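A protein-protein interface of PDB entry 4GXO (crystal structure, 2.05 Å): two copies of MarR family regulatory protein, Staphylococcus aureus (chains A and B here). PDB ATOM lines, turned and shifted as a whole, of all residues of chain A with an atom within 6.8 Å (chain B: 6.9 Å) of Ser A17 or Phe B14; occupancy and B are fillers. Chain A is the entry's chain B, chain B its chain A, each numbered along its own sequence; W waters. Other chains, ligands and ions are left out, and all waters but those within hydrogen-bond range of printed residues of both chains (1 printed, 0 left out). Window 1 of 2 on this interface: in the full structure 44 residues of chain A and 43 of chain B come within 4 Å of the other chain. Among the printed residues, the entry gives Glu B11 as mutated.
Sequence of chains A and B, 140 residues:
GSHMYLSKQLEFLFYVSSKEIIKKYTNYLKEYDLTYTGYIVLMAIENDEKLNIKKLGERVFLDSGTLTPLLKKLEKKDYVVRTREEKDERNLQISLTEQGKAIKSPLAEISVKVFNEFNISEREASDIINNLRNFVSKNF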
ATOM      1  N   PHE A  12     -15.926  -0.824 -23.723  1.00  0.00           N
ATOM      2  CA  PHE A  12     -16.447  -0.741 -22.380  1.00  0.00           C
ATOM      3  C   PHE A  12     -16.288  -2.058 -21.642  1.00  0.00           C
ATOM      4  O   PHE A  12     -15.737  -2.104 -20.527  1.00  0.00           O
ATOM      5  CB  PHE A  12     -17.920  -0.326 -22.411  1.00  0.00           C
ATOM      6  CG  PHE A  12     -18.540  -0.242 -21.045  1.00  0.00           C
ATOM      7  CD1 PHE A  12     -18.249   0.812 -20.217  1.00  0.00           C
ATOM      8  CD2 PHE A  12     -19.387  -1.242 -20.588  1.00  0.00           C
ATOM      9  CE1 PHE A  12     -18.792   0.888 -18.944  1.00  0.00           C
ATOM     10  CE2 PHE A  12     -19.942  -1.174 -19.325  1.00  0.00           C
ATOM     11  CZ  PHE A  12     -19.647  -0.102 -18.499  1.00  0.00           C
ATOM     12  N   LEU A  13     -16.722  -3.136 -22.288  1.00  0.00           N
ATOM     13  CA  LEU A  13     -16.784  -4.435 -21.634  1.00  0.00           C
ATOM     14  C   LEU A  13     -15.417  -5.044 -21.399  1.00  0.00           C
ATOM     15  O   LEU A  13     -15.202  -5.648 -20.345  1.00  0.00           O
ATOM     16  CB  LEU A  13     -17.711  -5.397 -22.394  1.00  0.00           C
ATOM     17  CG  LEU A  13     -19.158  -4.932 -22.272  1.00  0.00           C
ATOM     18  CD1 LEU A  13     -20.040  -5.576 -23.322  1.00  0.00           C
ATOM     19  CD2 LEU A  13     -19.716  -5.204 -20.879  1.00  0.00           C
ATOM     20  N   PHE A  14     -14.492  -4.901 -22.343  1.00  0.00           N
ATOM     21  CA  PHE A  14     -13.131  -5.352 -22.088  1.00  0.00           C
ATOM     22  C   PHE A  14     -12.505  -4.552 -20.946  1.00  0.00           C
ATOM     23  O   PHE A  14     -11.855  -5.121 -20.093  1.00  0.00           O
ATOM     24  CB  PHE A  14     -12.241  -5.245 -23.334  1.00  0.00           C
ATOM     25  CG  PHE A  14     -12.231  -6.480 -24.187  1.00  0.00           C
ATOM     26  CD1 PHE A  14     -11.566  -7.626 -23.770  1.00  0.00           C
ATOM     27  CD2 PHE A  14     -12.860  -6.490 -25.424  1.00  0.00           C
ATOM     28  CE1 PHE A  14     -11.542  -8.754 -24.569  1.00  0.00           C
ATOM     29  CE2 PHE A  14     -12.833  -7.617 -26.226  1.00  0.00           C
ATOM     30  CZ  PHE A  14     -12.161  -8.749 -25.796  1.00  0.00           C
ATOM     31  N   TYR A  15     -12.694  -3.236 -20.939  1.00  0.00           N
ATOM     32  CA  TYR A  15     -12.120  -2.380 -19.892  1.00  0.00           C
ATOM     33  C   TYR A  15     -12.641  -2.778 -18.492  1.00  0.00           C
ATOM     34  O   TYR A  15     -11.861  -3.060 -17.571  1.00  0.00           O
ATOM     35  CB  TYR A  15     -12.395  -0.889 -20.182  1.00  0.00           C
ATOM     36  CG  TYR A  15     -11.697   0.035 -19.207  1.00  0.00           C
ATOM     37  CD1 TYR A  15     -10.418   0.491 -19.465  1.00  0.00           C
ATOM     38  CD2 TYR A  15     -12.304   0.426 -18.014  1.00  0.00           C
ATOM     39  CE1 TYR A  15      -9.743   1.306 -18.560  1.00  0.00           C
ATOM     40  CE2 TYR A  15     -11.640   1.251 -17.107  1.00  0.00           C
ATOM     41  CZ  TYR A  15     -10.365   1.690 -17.394  1.00  0.00           C
ATOM     42  OH  TYR A  15      -9.690   2.516 -16.532  1.00  0.00           O
ATOM     43  N   VAL A  16     -13.956  -2.843 -18.343  1.00  0.00           N
ATOM     44  CA  VAL A  16     -14.559  -3.150 -17.044  1.00  0.00           C
ATOM     45  C   VAL A  16     -14.239  -4.593 -16.597  1.00  0.00           C
ATOM     46  O   VAL A  16     -13.902  -4.824 -15.431  1.00  0.00           O
ATOM     47  CB  VAL A  16     -16.073  -2.842 -17.036  1.00  0.00           C
ATOM     48  CG1 VAL A  16     -16.714  -3.241 -15.711  1.00  0.00           C
ATOM     49  CG2 VAL A  16     -16.301  -1.358 -17.281  1.00  0.00           C
ATOM     50  N   SER A  17     -14.323  -5.537 -17.530  1.00  0.00           N
ATOM     51  CA  SER A  17     -13.940  -6.924 -17.299  1.00  0.00           C
ATOM     52  C   SER A  17     -12.563  -7.052 -16.672  1.00  0.00           C
ATOM     53  O   SER A  17     -12.396  -7.619 -15.587  1.00  0.00           O
ATOM     54  CB  SER A  17     -13.932  -7.703 -18.621  1.00  0.00           C
ATOM     55  OG  SER A  17     -15.226  -8.199 -18.862  1.00  0.00           O
ATOM     56  N   SER A  18     -11.574  -6.526 -17.373  1.00  0.00           N
ATOM     57  CA  SER A  18     -10.200  -6.663 -16.931  1.00  0.00           C
ATOM     58  C   SER A  18      -9.963  -5.923 -15.609  1.00  0.00           C
ATOM     59  O   SER A  18      -9.221  -6.397 -14.742  1.00  0.00           O
ATOM     60  CB  SER A  18      -9.263  -6.171 -18.033  1.00  0.00           C
ATOM     61  OG  SER A  18      -9.575  -4.844 -18.360  1.00  0.00           O
ATOM     62  N   LYS A  19     -10.598  -4.772 -15.431  1.00  0.00           N
ATOM     63  CA  LYS A  19     -10.440  -4.012 -14.193  1.00  0.00           C
ATOM     64  C   LYS A  19     -11.112  -4.713 -12.993  1.00  0.00           C
ATOM     65  O   LYS A  19     -10.584  -4.680 -11.885  1.00  0.00           O
ATOM     66  CB  LYS A  19     -10.981  -2.581 -14.335  1.00  0.00           C
ATOM     67  CG  LYS A  19     -10.181  -1.682 -15.277  1.00  0.00           C
ATOM     68  CD  LYS A  19      -8.674  -1.878 -15.134  1.00  0.00           C
ATOM     69  CE  LYS A  19      -7.877  -0.735 -15.747  1.00  0.00           C
ATOM     70  NZ  LYS A  19      -7.743   0.433 -14.831  1.00  0.00           N
ATOM     71  N   GLU A  20     -12.255  -5.351 -13.214  1.00  0.00           N
ATOM     72  CA  GLU A  20     -12.934  -6.085 -12.137  1.00  0.00           C
ATOM     73  C   GLU A  20     -12.114  -7.307 -11.749  1.00  0.00           C
ATOM     74  O   GLU A  20     -11.973  -7.614 -10.575  1.00  0.00           O
ATOM     75  CB  GLU A  20     -14.369  -6.469 -12.540  1.00  0.00           C
ATOM     76  CG  GLU A  20     -15.308  -5.260 -12.558  1.00  0.00           C
ATOM     77  CD  GLU A  20     -16.765  -5.593 -12.884  1.00  0.00           C
ATOM     78  OE1 GLU A  20     -17.100  -6.768 -13.125  1.00  0.00           O
ATOM     79  OE2 GLU A  20     -17.597  -4.654 -12.896  1.00  0.00           O
ATOM     80  N   ILE A  21     -11.545  -7.980 -12.743  1.00  0.00           N
ATOM     81  CA  ILE A  21     -10.634  -9.098 -12.500  1.00  0.00           C
ATOM     82  C   ILE A  21      -9.427  -8.668 -11.648  1.00  0.00           C
ATOM     83  O   ILE A  21      -9.140  -9.277 -10.611  1.00  0.00           O
ATOM     84  CB  ILE A  21     -10.158  -9.716 -13.825  1.00  0.00           C
ATOM     85  CG1 ILE A  21     -11.303 -10.495 -14.479  1.00  0.00           C
ATOM     86  CG2 ILE A  21      -8.951 -10.633 -13.618  1.00  0.00           C
ATOM     87  CD1 ILE A  21     -11.073 -10.783 -15.955  1.00  0.00           C
ATOM     88  N   ILE A  22      -8.737  -7.623 -12.098  1.00  0.00           N
ATOM     89  CA  ILE A  22      -7.563  -7.124 -11.437  1.00  0.00           C
ATOM     90  C   ILE A  22      -7.843  -6.672 -10.012  1.00  0.00           C
ATOM     91  O   ILE A  22      -7.026  -6.892  -9.126  1.00  0.00           O
ATOM     92  CB  ILE A  22      -6.890  -5.986 -12.241  1.00  0.00           C
ATOM     93  CG1 ILE A  22      -6.266  -6.561 -13.513  1.00  0.00           C
ATOM     94  CG2 ILE A  22      -5.798  -5.303 -11.405  1.00  0.00           C
ATOM     95  CD1 ILE A  22      -6.039  -5.550 -14.602  1.00  0.00           C
ATOM     96  N   TYR A  36      -0.710  -7.036  -8.538  1.00  0.00           N
ATOM     97  CA  TYR A  36      -1.113  -7.911  -9.636  1.00  0.00           C
ATOM     98  C   TYR A  36       0.005  -8.106 -10.652  1.00  0.00           C
ATOM     99  O   TYR A  36       0.281  -9.224 -11.079  1.00  0.00           O
ATOM    100  CB  TYR A  36      -2.342  -7.329 -10.318  1.00  0.00           C
ATOM    101  CG  TYR A  36      -2.763  -8.031 -11.577  1.00  0.00           C
ATOM    102  CD1 TYR A  36      -3.409  -9.253 -11.526  1.00  0.00           C
ATOM    103  CD2 TYR A  36      -2.528  -7.460 -12.821  1.00  0.00           C
ATOM    104  CE1 TYR A  36      -3.804  -9.898 -12.680  1.00  0.00           C
ATOM    105  CE2 TYR A  36      -2.918  -8.101 -13.982  1.00  0.00           C
ATOM    106  CZ  TYR A  36      -3.562  -9.309 -13.905  1.00  0.00           C
ATOM    107  OH  TYR A  36      -3.954  -9.945 -15.052  1.00  0.00           O
ATOM    108  N   PHE A 115     -11.815 -16.141 -10.160  1.00  0.00           N
ATOM    109  CA  PHE A 115     -12.817 -16.403 -11.191  1.00  0.00           C
ATOM    110  C   PHE A 115     -14.078 -17.084 -10.670  1.00  0.00           C
ATOM    111  O   PHE A 115     -15.150 -16.858 -11.225  1.00  0.00           O
ATOM    112  CB  PHE A 115     -12.200 -17.107 -12.413  1.00  0.00           C
ATOM    113  CG  PHE A 115     -11.417 -16.170 -13.271  1.00  0.00           C
ATOM    114  CD1 PHE A 115     -12.073 -15.322 -14.154  1.00  0.00           C
ATOM    115  CD2 PHE A 115     -10.035 -16.069 -13.152  1.00  0.00           C
ATOM    116  CE1 PHE A 115     -11.363 -14.407 -14.920  1.00  0.00           C
ATOM    117  CE2 PHE A 115      -9.330 -15.162 -13.911  1.00  0.00           C
ATOM    118  CZ  PHE A 115      -9.995 -14.328 -14.791  1.00  0.00           C
ATOM    119  N   PHE A 118     -17.020 -14.742  -9.982  1.00  0.00           N
ATOM    120  CA  PHE A 118     -17.878 -14.251 -11.055  1.00  0.00           C
ATOM    121  C   PHE A 118     -19.069 -15.171 -11.258  1.00  0.00           C
ATOM    122  O   PHE A 118     -20.079 -14.756 -11.821  1.00  0.00           O
ATOM    123  CB  PHE A 118     -17.089 -14.051 -12.346  1.00  0.00           C
ATOM    124  CG  PHE A 118     -16.178 -12.866 -12.298  1.00  0.00           C
ATOM    125  CD1 PHE A 118     -14.861 -13.007 -11.886  1.00  0.00           C
ATOM    126  CD2 PHE A 118     -16.654 -11.591 -12.623  1.00  0.00           C
ATOM    127  CE1 PHE A 118     -14.019 -11.912 -11.824  1.00  0.00           C
ATOM    128  CE2 PHE A 118     -15.824 -10.491 -12.554  1.00  0.00           C
ATOM    129  CZ  PHE A 118     -14.498 -10.649 -12.165  1.00  0.00           C
ATOM    130  N   ILE A 128     -16.304 -17.947 -23.185  1.00  0.00           N
ATOM    131  CA  ILE A 128     -15.448 -16.787 -23.067  1.00  0.00           C
ATOM    132  C   ILE A 128     -14.018 -17.110 -23.525  1.00  0.00           C
ATOM    133  O   ILE A 128     -13.388 -16.308 -24.228  1.00  0.00           O
ATOM    134  CB  ILE A 128     -15.438 -16.228 -21.632  1.00  0.00           C
ATOM    135  CG1 ILE A 128     -16.746 -15.493 -21.336  1.00  0.00           C
ATOM    136  CG2 ILE A 128     -14.288 -15.257 -21.460  1.00  0.00           C
ATOM    137  CD1 ILE A 128     -17.104 -15.475 -19.855  1.00  0.00           C
ATOM    138  N   LEU A 132     -12.205 -15.268 -26.635  1.00  0.00           N
ATOM    139  CA  LEU A 132     -11.001 -14.479 -26.426  1.00  0.00           C
ATOM    140  C   LEU A 132      -9.796 -15.050 -27.161  1.00  0.00           C
ATOM    141  O   LEU A 132      -8.901 -14.290 -27.545  1.00  0.00           O
ATOM    142  CB  LEU A 132     -10.662 -14.346 -24.939  1.00  0.00           C
ATOM    143  CG  LEU A 132     -11.659 -13.600 -24.046  1.00  0.00           C
ATOM    144  CD1 LEU A 132     -11.275 -13.757 -22.589  1.00  0.00           C
ATOM    145  CD2 LEU A 132     -11.722 -12.135 -24.428  1.00  0.00           C
ATOM    146  N   VAL A 136      -7.652 -13.095 -29.829  1.00  0.00           N
ATOM    147  CA  VAL A 136      -6.183 -12.923 -29.738  1.00  0.00           C
ATOM    148  C   VAL A 136      -5.411 -13.514 -30.947  1.00  0.00           C
ATOM    149  O   VAL A 136      -4.184 -13.379 -31.041  1.00  0.00           O
ATOM    150  CB  VAL A 136      -5.676 -13.495 -28.381  1.00  0.00           C
ATOM    151  CG1 VAL A 136      -4.161 -13.636 -28.311  1.00  0.00           C
ATOM    152  CG2 VAL A 136      -6.152 -12.610 -27.233  1.00  0.00           C
ATOM    153  N   GLN B   9      -6.643 -20.298 -18.053  1.00  0.00           N
ATOM    154  CA  GLN B   9      -6.907 -19.860 -19.416  1.00  0.00           C
ATOM    155  C   GLN B   9      -7.538 -18.473 -19.403  1.00  0.00           C
ATOM    156  O   GLN B   9      -7.116 -17.585 -20.141  1.00  0.00           O
ATOM    157  CB  GLN B   9      -7.825 -20.835 -20.169  1.00  0.00           C
ATOM    158  CG  GLN B   9      -7.255 -22.220 -20.424  1.00  0.00           C
ATOM    159  CD  GLN B   9      -5.942 -22.189 -21.168  1.00  0.00           C
ATOM    160  OE1 GLN B   9      -5.900 -21.988 -22.388  1.00  0.00           O
ATOM    161  NE2 GLN B   9      -4.849 -22.397 -20.439  1.00  0.00           N
ATOM    162  N   LEU B  10      -8.533 -18.291 -18.544  1.00  0.00           N
ATOM    163  CA  LEU B  10      -9.223 -17.024 -18.432  1.00  0.00           C
ATOM    164  C   LEU B  10      -8.252 -15.924 -18.024  1.00  0.00           C
ATOM    165  O   LEU B  10      -8.248 -14.853 -18.616  1.00  0.00           O
ATOM    166  CB  LEU B  10     -10.393 -17.128 -17.427  1.00  0.00           C
ATOM    167  CG  LEU B  10     -11.630 -17.943 -17.858  1.00  0.00           C
ATOM    168  CD1 LEU B  10     -12.508 -18.261 -16.656  1.00  0.00           C
ATOM    169  CD2 LEU B  10     -12.442 -17.239 -18.921  1.00  0.00           C
ATOM    170  N   GLU B  11      -7.437 -16.191 -17.005  1.00  0.00           N
ATOM    171  CA  GLU B  11      -6.462 -15.208 -16.541  1.00  0.00           C
ATOM    172  C   GLU B  11      -5.546 -14.782 -17.677  1.00  0.00           C
ATOM    173  O   GLU B  11      -5.338 -13.583 -17.918  1.00  0.00           O
ATOM    174  CB  GLU B  11      -5.613 -15.794 -15.402  1.00  0.00           C
ATOM    175  CG  GLU B  11      -4.505 -14.869 -14.939  1.00  0.00           C
ATOM    176  CD  GLU B  11      -3.499 -15.561 -14.051  1.00  0.00           C
ATOM    177  OE1 GLU B  11      -3.859 -15.994 -12.939  1.00  0.00           O
ATOM    178  OE2 GLU B  11      -2.342 -15.674 -14.473  1.00  0.00           O
ATOM    179  N   PHE B  12      -4.970 -15.770 -18.352  1.00  0.00           N
ATOM    180  CA  PHE B  12      -4.043 -15.520 -19.460  1.00  0.00           C
ATOM    181  C   PHE B  12      -4.688 -14.718 -20.569  1.00  0.00           C
ATOM    182  O   PHE B  12      -4.137 -13.714 -20.998  1.00  0.00           O
ATOM    183  CB  PHE B  12      -3.489 -16.843 -20.016  1.00  0.00           C
ATOM    184  CG  PHE B  12      -2.665 -16.695 -21.271  1.00  0.00           C
ATOM    185  CD1 PHE B  12      -1.336 -16.309 -21.211  1.00  0.00           C
ATOM    186  CD2 PHE B  12      -3.212 -16.976 -22.514  1.00  0.00           C
ATOM    187  CE1 PHE B  12      -0.565 -16.195 -22.366  1.00  0.00           C
ATOM    188  CE2 PHE B  12      -2.451 -16.858 -23.672  1.00  0.00           C
ATOM    189  CZ  PHE B  12      -1.131 -16.464 -23.598  1.00  0.00           C
ATOM    190  N   LEU B  13      -5.845 -15.177 -21.041  1.00  0.00           N
ATOM    191  CA  LEU B  13      -6.524 -14.550 -22.184  1.00  0.00           C
ATOM    192  C   LEU B  13      -7.062 -13.143 -21.898  1.00  0.00           C
ATOM    193  O   LEU B  13      -7.021 -12.283 -22.773  1.00  0.00           O
ATOM    194  CB  LEU B  13      -7.641 -15.465 -22.710  1.00  0.00           C
ATOM    195  CG  LEU B  13      -7.068 -16.748 -23.339  1.00  0.00           C
ATOM    196  CD1 LEU B  13      -8.115 -17.838 -23.478  1.00  0.00           C
ATOM    197  CD2 LEU B  13      -6.425 -16.453 -24.694  1.00  0.00           C
ATOM    198  N   PHE B  14      -7.560 -12.899 -20.688  1.00  0.00           N
ATOM    199  CA  PHE B  14      -7.947 -11.537 -20.308  1.00  0.00           C
ATOM    200  C   PHE B  14      -6.707 -10.624 -20.237  1.00  0.00           C
ATOM    201  O   PHE B  14      -6.757  -9.457 -20.656  1.00  0.00           O
ATOM    202  CB  PHE B  14      -8.722 -11.536 -18.980  1.00  0.00           C
ATOM    203  CG  PHE B  14     -10.213 -11.708 -19.134  1.00  0.00           C
ATOM    204  CD1 PHE B  14     -10.988 -10.689 -19.681  1.00  0.00           C
ATOM    205  CD2 PHE B  14     -10.843 -12.847 -18.690  1.00  0.00           C
ATOM    206  CE1 PHE B  14     -12.362 -10.824 -19.797  1.00  0.00           C
ATOM    207  CE2 PHE B  14     -12.223 -12.989 -18.802  1.00  0.00           C
ATOM    208  CZ  PHE B  14     -12.977 -11.965 -19.361  1.00  0.00           C
ATOM    209  N   TYR B  15      -5.584 -11.170 -19.757  1.00  0.00           N
ATOM    210  CA  TYR B  15      -4.338 -10.412 -19.658  1.00  0.00           C
ATOM    211  C   TYR B  15      -3.801 -10.040 -21.052  1.00  0.00           C
ATOM    212  O   TYR B  15      -3.469  -8.885 -21.317  1.00  0.00           O
ATOM    213  CB  TYR B  15      -3.270 -11.201 -18.857  1.00  0.00           C
ATOM    214  CG  TYR B  15      -1.974 -10.428 -18.651  1.00  0.00           C
ATOM    215  CD1 TYR B  15      -1.842  -9.531 -17.603  1.00  0.00           C
ATOM    216  CD2 TYR B  15      -0.891 -10.590 -19.510  1.00  0.00           C
ATOM    217  CE1 TYR B  15      -0.667  -8.800 -17.415  1.00  0.00           C
ATOM    218  CE2 TYR B  15       0.283  -9.871 -19.328  1.00  0.00           C
ATOM    219  CZ  TYR B  15       0.390  -8.982 -18.273  1.00  0.00           C
ATOM    220  OH  TYR B  15       1.542  -8.251 -18.083  1.00  0.00           O
ATOM    221  N   VAL B  16      -3.721 -11.023 -21.941  1.00  0.00           N
ATOM    222  CA  VAL B  16      -3.158 -10.780 -23.258  1.00  0.00           C
ATOM    223  C   VAL B  16      -4.096  -9.949 -24.164  1.00  0.00           C
ATOM    224  O   VAL B  16      -3.594  -9.135 -24.943  1.00  0.00           O
ATOM    225  CB  VAL B  16      -2.711 -12.095 -23.945  1.00  0.00           C
ATOM    226  CG1 VAL B  16      -2.160 -11.823 -25.342  1.00  0.00           C
ATOM    227  CG2 VAL B  16      -1.645 -12.792 -23.109  1.00  0.00           C
ATOM    228  N   SER B  17      -5.415 -10.134 -24.074  1.00  0.00           N
ATOM    229  CA  SER B  17      -6.342  -9.319 -24.882  1.00  0.00           C
ATOM    230  C   SER B  17      -6.292  -7.852 -24.444  1.00  0.00           C
ATOM    231  O   SER B  17      -6.342  -6.950 -25.274  1.00  0.00           O
ATOM    232  CB  SER B  17      -7.784  -9.845 -24.815  1.00  0.00           C
ATOM    233  OG  SER B  17      -8.203 -10.113 -23.492  1.00  0.00           O
ATOM    234  N   SER B  18      -6.192  -7.622 -23.139  1.00  0.00           N
ATOM    235  CA  SER B  18      -6.047  -6.274 -22.616  1.00  0.00           C
ATOM    236  C   SER B  18      -4.745  -5.617 -23.109  1.00  0.00           C
ATOM    237  O   SER B  18      -4.769  -4.468 -23.545  1.00  0.00           O
ATOM    238  CB  SER B  18      -6.111  -6.297 -21.086  1.00  0.00           C
ATOM    239  OG  SER B  18      -5.581  -5.104 -20.560  1.00  0.00           O
ATOM    240  N   LYS B  19      -3.632  -6.352 -23.096  1.00  0.00           N
ATOM    241  CA  LYS B  19      -2.378  -5.807 -23.634  1.00  0.00           C
ATOM    242  C   LYS B  19      -2.468  -5.504 -25.137  1.00  0.00           C
ATOM    243  O   LYS B  19      -1.966  -4.471 -25.592  1.00  0.00           O
ATOM    244  CB  LYS B  19      -1.188  -6.737 -23.383  1.00  0.00           C
ATOM    245  CG  LYS B  19      -0.792  -6.874 -21.921  1.00  0.00           C
ATOM    246  CD  LYS B  19      -0.277  -5.582 -21.295  1.00  0.00           C
ATOM    247  CE  LYS B  19       0.251  -5.821 -19.890  1.00  0.00           C
ATOM    248  NZ  LYS B  19      -0.146  -4.752 -18.930  1.00  0.00           N
ATOM    249  N   PHE B  61     -11.836   2.819 -12.429  1.00  0.00           N
ATOM    250  CA  PHE B  61     -11.052   1.839 -11.666  1.00  0.00           C
ATOM    251  C   PHE B  61      -9.614   2.303 -11.464  1.00  0.00           C
ATOM    252  O   PHE B  61      -8.650   1.548 -11.674  1.00  0.00           O
ATOM    253  CB  PHE B  61     -11.098   0.449 -12.332  1.00  0.00           C
ATOM    254  CG  PHE B  61     -12.480  -0.165 -12.372  1.00  0.00           C
ATOM    255  CD1 PHE B  61     -12.848  -1.147 -11.454  1.00  0.00           C
ATOM    256  CD2 PHE B  61     -13.415   0.249 -13.315  1.00  0.00           C
ATOM    257  CE1 PHE B  61     -14.118  -1.716 -11.493  1.00  0.00           C
ATOM    258  CE2 PHE B  61     -14.681  -0.307 -13.354  1.00  0.00           C
ATOM    259  CZ  PHE B  61     -15.033  -1.292 -12.442  1.00  0.00           C
ATOM    260  N   ASN B 131     -21.285 -12.295 -23.948  1.00  0.00           N
ATOM    261  CA  ASN B 131     -20.615 -13.075 -22.904  1.00  0.00           C
ATOM    262  C   ASN B 131     -19.947 -12.205 -21.841  1.00  0.00           C
ATOM    263  O   ASN B 131     -20.006 -12.511 -20.655  1.00  0.00           O
ATOM    264  CB  ASN B 131     -19.636 -14.085 -23.504  1.00  0.00           C
ATOM    265  CG  ASN B 131     -20.334 -15.204 -24.265  1.00  0.00           C
ATOM    266  OD1 ASN B 131     -19.748 -15.837 -25.135  1.00  0.00           O
ATOM    267  ND2 ASN B 131     -21.567 -15.462 -23.930  1.00  0.00           N
ATOM    268  N   LEU B 132     -19.325 -11.119 -22.256  1.00  0.00           N
ATOM    269  CA  LEU B 132     -18.704 -10.195 -21.308  1.00  0.00           C
ATOM    270  C   LEU B 132     -19.726  -9.399 -20.524  1.00  0.00           C
ATOM    271  O   LEU B 132     -19.474  -9.019 -19.386  1.00  0.00           O
ATOM    272  CB  LEU B 132     -17.774  -9.234 -22.024  1.00  0.00           C
ATOM    273  CG  LEU B 132     -16.497  -9.885 -22.542  1.00  0.00           C
ATOM    274  CD1 LEU B 132     -15.573  -8.782 -23.021  1.00  0.00           C
ATOM    275  CD2 LEU B 132     -15.802 -10.794 -21.547  1.00  0.00           C
ATOM    276  N   ARG B 133     -20.875  -9.128 -21.131  1.00  0.00           N
ATOM    277  CA  ARG B 133     -21.944  -8.439 -20.434  1.00  0.00           C
ATOM    278  C   ARG B 133     -22.470  -9.302 -19.282  1.00  0.00           C
ATOM    279  O   ARG B 133     -22.685  -8.806 -18.171  1.00  0.00           O
ATOM    280  CB  ARG B 133     -23.061  -8.105 -21.416  1.00  0.00           C
ATOM    281  CG  ARG B 133     -24.097  -7.140 -20.879  1.00  0.00           C
ATOM    282  CD  ARG B 133     -25.090  -6.843 -21.986  1.00  0.00           C
ATOM    283  NE  ARG B 133     -24.647  -5.779 -22.874  1.00  0.00           N
ATOM    284  CZ  ARG B 133     -24.940  -5.695 -24.166  1.00  0.00           C
ATOM    285  NH1 ARG B 133     -25.671  -6.624 -24.766  1.00  0.00           N
ATOM    286  NH2 ARG B 133     -24.515  -4.650 -24.846  1.00  0.00           N
ATOM    287  N   PHE B 135     -20.677 -11.686 -17.770  1.00  0.00           N
ATOM    288  CA  PHE B 135     -19.539 -11.744 -16.815  1.00  0.00           C
ATOM    289  C   PHE B 135     -19.512 -10.557 -15.838  1.00  0.00           C
ATOM    290  O   PHE B 135     -19.554 -10.725 -14.621  1.00  0.00           O
ATOM    291  CB  PHE B 135     -18.247 -11.797 -17.649  1.00  0.00           C
ATOM    292  CG  PHE B 135     -16.987 -12.036 -16.854  1.00  0.00           C
ATOM    293  CD1 PHE B 135     -16.081 -11.011 -16.649  1.00  0.00           C
ATOM    294  CD2 PHE B 135     -16.705 -13.287 -16.328  1.00  0.00           C
ATOM    295  CE1 PHE B 135     -14.909 -11.226 -15.932  1.00  0.00           C
ATOM    296  CE2 PHE B 135     -15.533 -13.518 -15.622  1.00  0.00           C
ATOM    297  CZ  PHE B 135     -14.640 -12.489 -15.421  1.00  0.00           C
ATOM    298  N   VAL B 136     -19.462  -9.358 -16.392  1.00  0.00           N
ATOM    299  CA  VAL B 136     -19.423  -8.105 -15.638  1.00  0.00           C
ATOM    300  C   VAL B 136     -20.653  -7.840 -14.731  1.00  0.00           C
ATOM    301  O   VAL B 136     -20.535  -7.149 -13.709  1.00  0.00           O
ATOM    302  CB  VAL B 136     -19.233  -6.945 -16.652  1.00  0.00           C
ATOM    303  CG1 VAL B 136     -19.738  -5.606 -16.145  1.00  0.00           C
ATOM    304  CG2 VAL B 136     -17.777  -6.880 -17.090  1.00  0.00           C
HETATM  305  O   HOH W   1      -6.338 -11.745 -16.001  1.00  0.00           O
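The backbone carbonyl oxygen of Phe B61 lies within hydrogen-bond range of the side-chain amino group of Lys A19 (3.5 Å).
The backbone carbonyl oxygen of Phe B14 lies within hydrogen-bond range of the side-chain hydroxyl of Ser B17, at 3.3 Å. The side-chain hydroxyl (OG) of Ser A17 is in hydrogen-bond range of the backbone carbonyl oxygen (O) of Leu A13. The side-chain hydroxyl (OH) of Tyr A15 is in hydrogen-bond range of the side-chain amino group (NZ) of Lys A19, at 3.3 Å.
Among the printed residues, pairs that only touch across the chains: Tyr A36 with Tyr B15 (3.3 Å), Ser A17 with Val B136 (3.4 Å), Ile A21 with Phe B14 (3.4 Å), Phe A118 with Phe B135 (3.4 Å), Glu A20 with Val B136 (3.5 Å), Ser A17 with Phe B135 (3.7 Å), Ser A17 with Phe B14 (3.7 Å), Ile A128 with Leu B10 (3.7 Å), Phe A14 with Ser B17 (3.8 Å), Phe A115 with Glu B11 (3.8 Å), Ser A17 with Leu B132 (3.8 Å), Phe A115 with Leu B10 (3.8 Å), Phe A115 with Phe B135 (3.8 Å), Leu A13 with Leu B132 (3.9 Å), Ile A21 with Phe B135 (3.9 Å), Val A16 with Val B136 (3.9 Å), Ile A128 with Asn B131 (3.9 Å), Glu A20 with Phe B61 (3.9 Å), Leu A132 with Leu B13 (3.9 Å), Leu A13 with Arg B133 (3.95 Å) and Leu A132 with Phe B14 (3.98 Å).
Ser A17 touches four residues of chain B. Phe B14 touches just these residues of chain A: Ser A17 (3.7 Å), Ile A21 (3.4 Å) and Leu A132 (3.98 Å). Printed residues of chain B within 4 Å of Lys A19: Phe B61. Of the printed residues of chain A, Asn B131 touches Ile A128 (3.9 Å). Of the printed residues of chain B, Tyr A36 touches Tyr B15 (3.3 Å). Val A136 touches none of the printed residues of chain B. Ser A18 touches none of the printed residues of chain B. The nearest residue of chain B that does not touch Ser A17 is Arg B133 (6.2 Å). The nearest residue of chain A that does not touch Phe B14 is Ile A128 (4.1 Å).
Of the 17 printed residues of chain A, 12 touch a printed residue of chain B. Hydrophobic or aromatic side chains of chain A that line the printed part of chain B: Leu A13, Phe A14, Val A16, Ile A21, Tyr A36, Phe A115, Phe A118, Ile A128 and Leu A132. Printed residues of chain B that touch a printed residue of chain A: Leu B10, Glu B11, Leu B13, Phe B14, Tyr B15, Ser B17, Phe B61, Asn B131, Leu B132, Arg B133, Phe B135 and Val B136. Hydrophobic or aromatic side chains of chain B that line the printed part of chain A: Leu B10, Leu B13, Phe B14, Tyr B15, Phe B61, Leu B132, Phe B135 and Val B136. Among the printed residues, 22 pairs touch across the chains. Among the printed residues, no Asp or Glu carboxylate lies within 4 Å of a Lys or Arg side-chain nitrogen of the other chain.
Leu A13 touches Leu B132, and with the chains exchanged Leu A132 touches Leu B13. Ser A17 touches Val B136, but with the chains exchanged Val A136 does not touch Ser B17 (4.02 Å). Positions printed for both chains: 12, 13, 14, 15, 16, 17, 18, 19, 132 and 136.
Water W1 lies within hydrogen-bond range of the backbone carbonyl oxygen of Glu B11 (2.8 Å) and the side-chain hydroxyl of Tyr A36 (3.1 Å).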
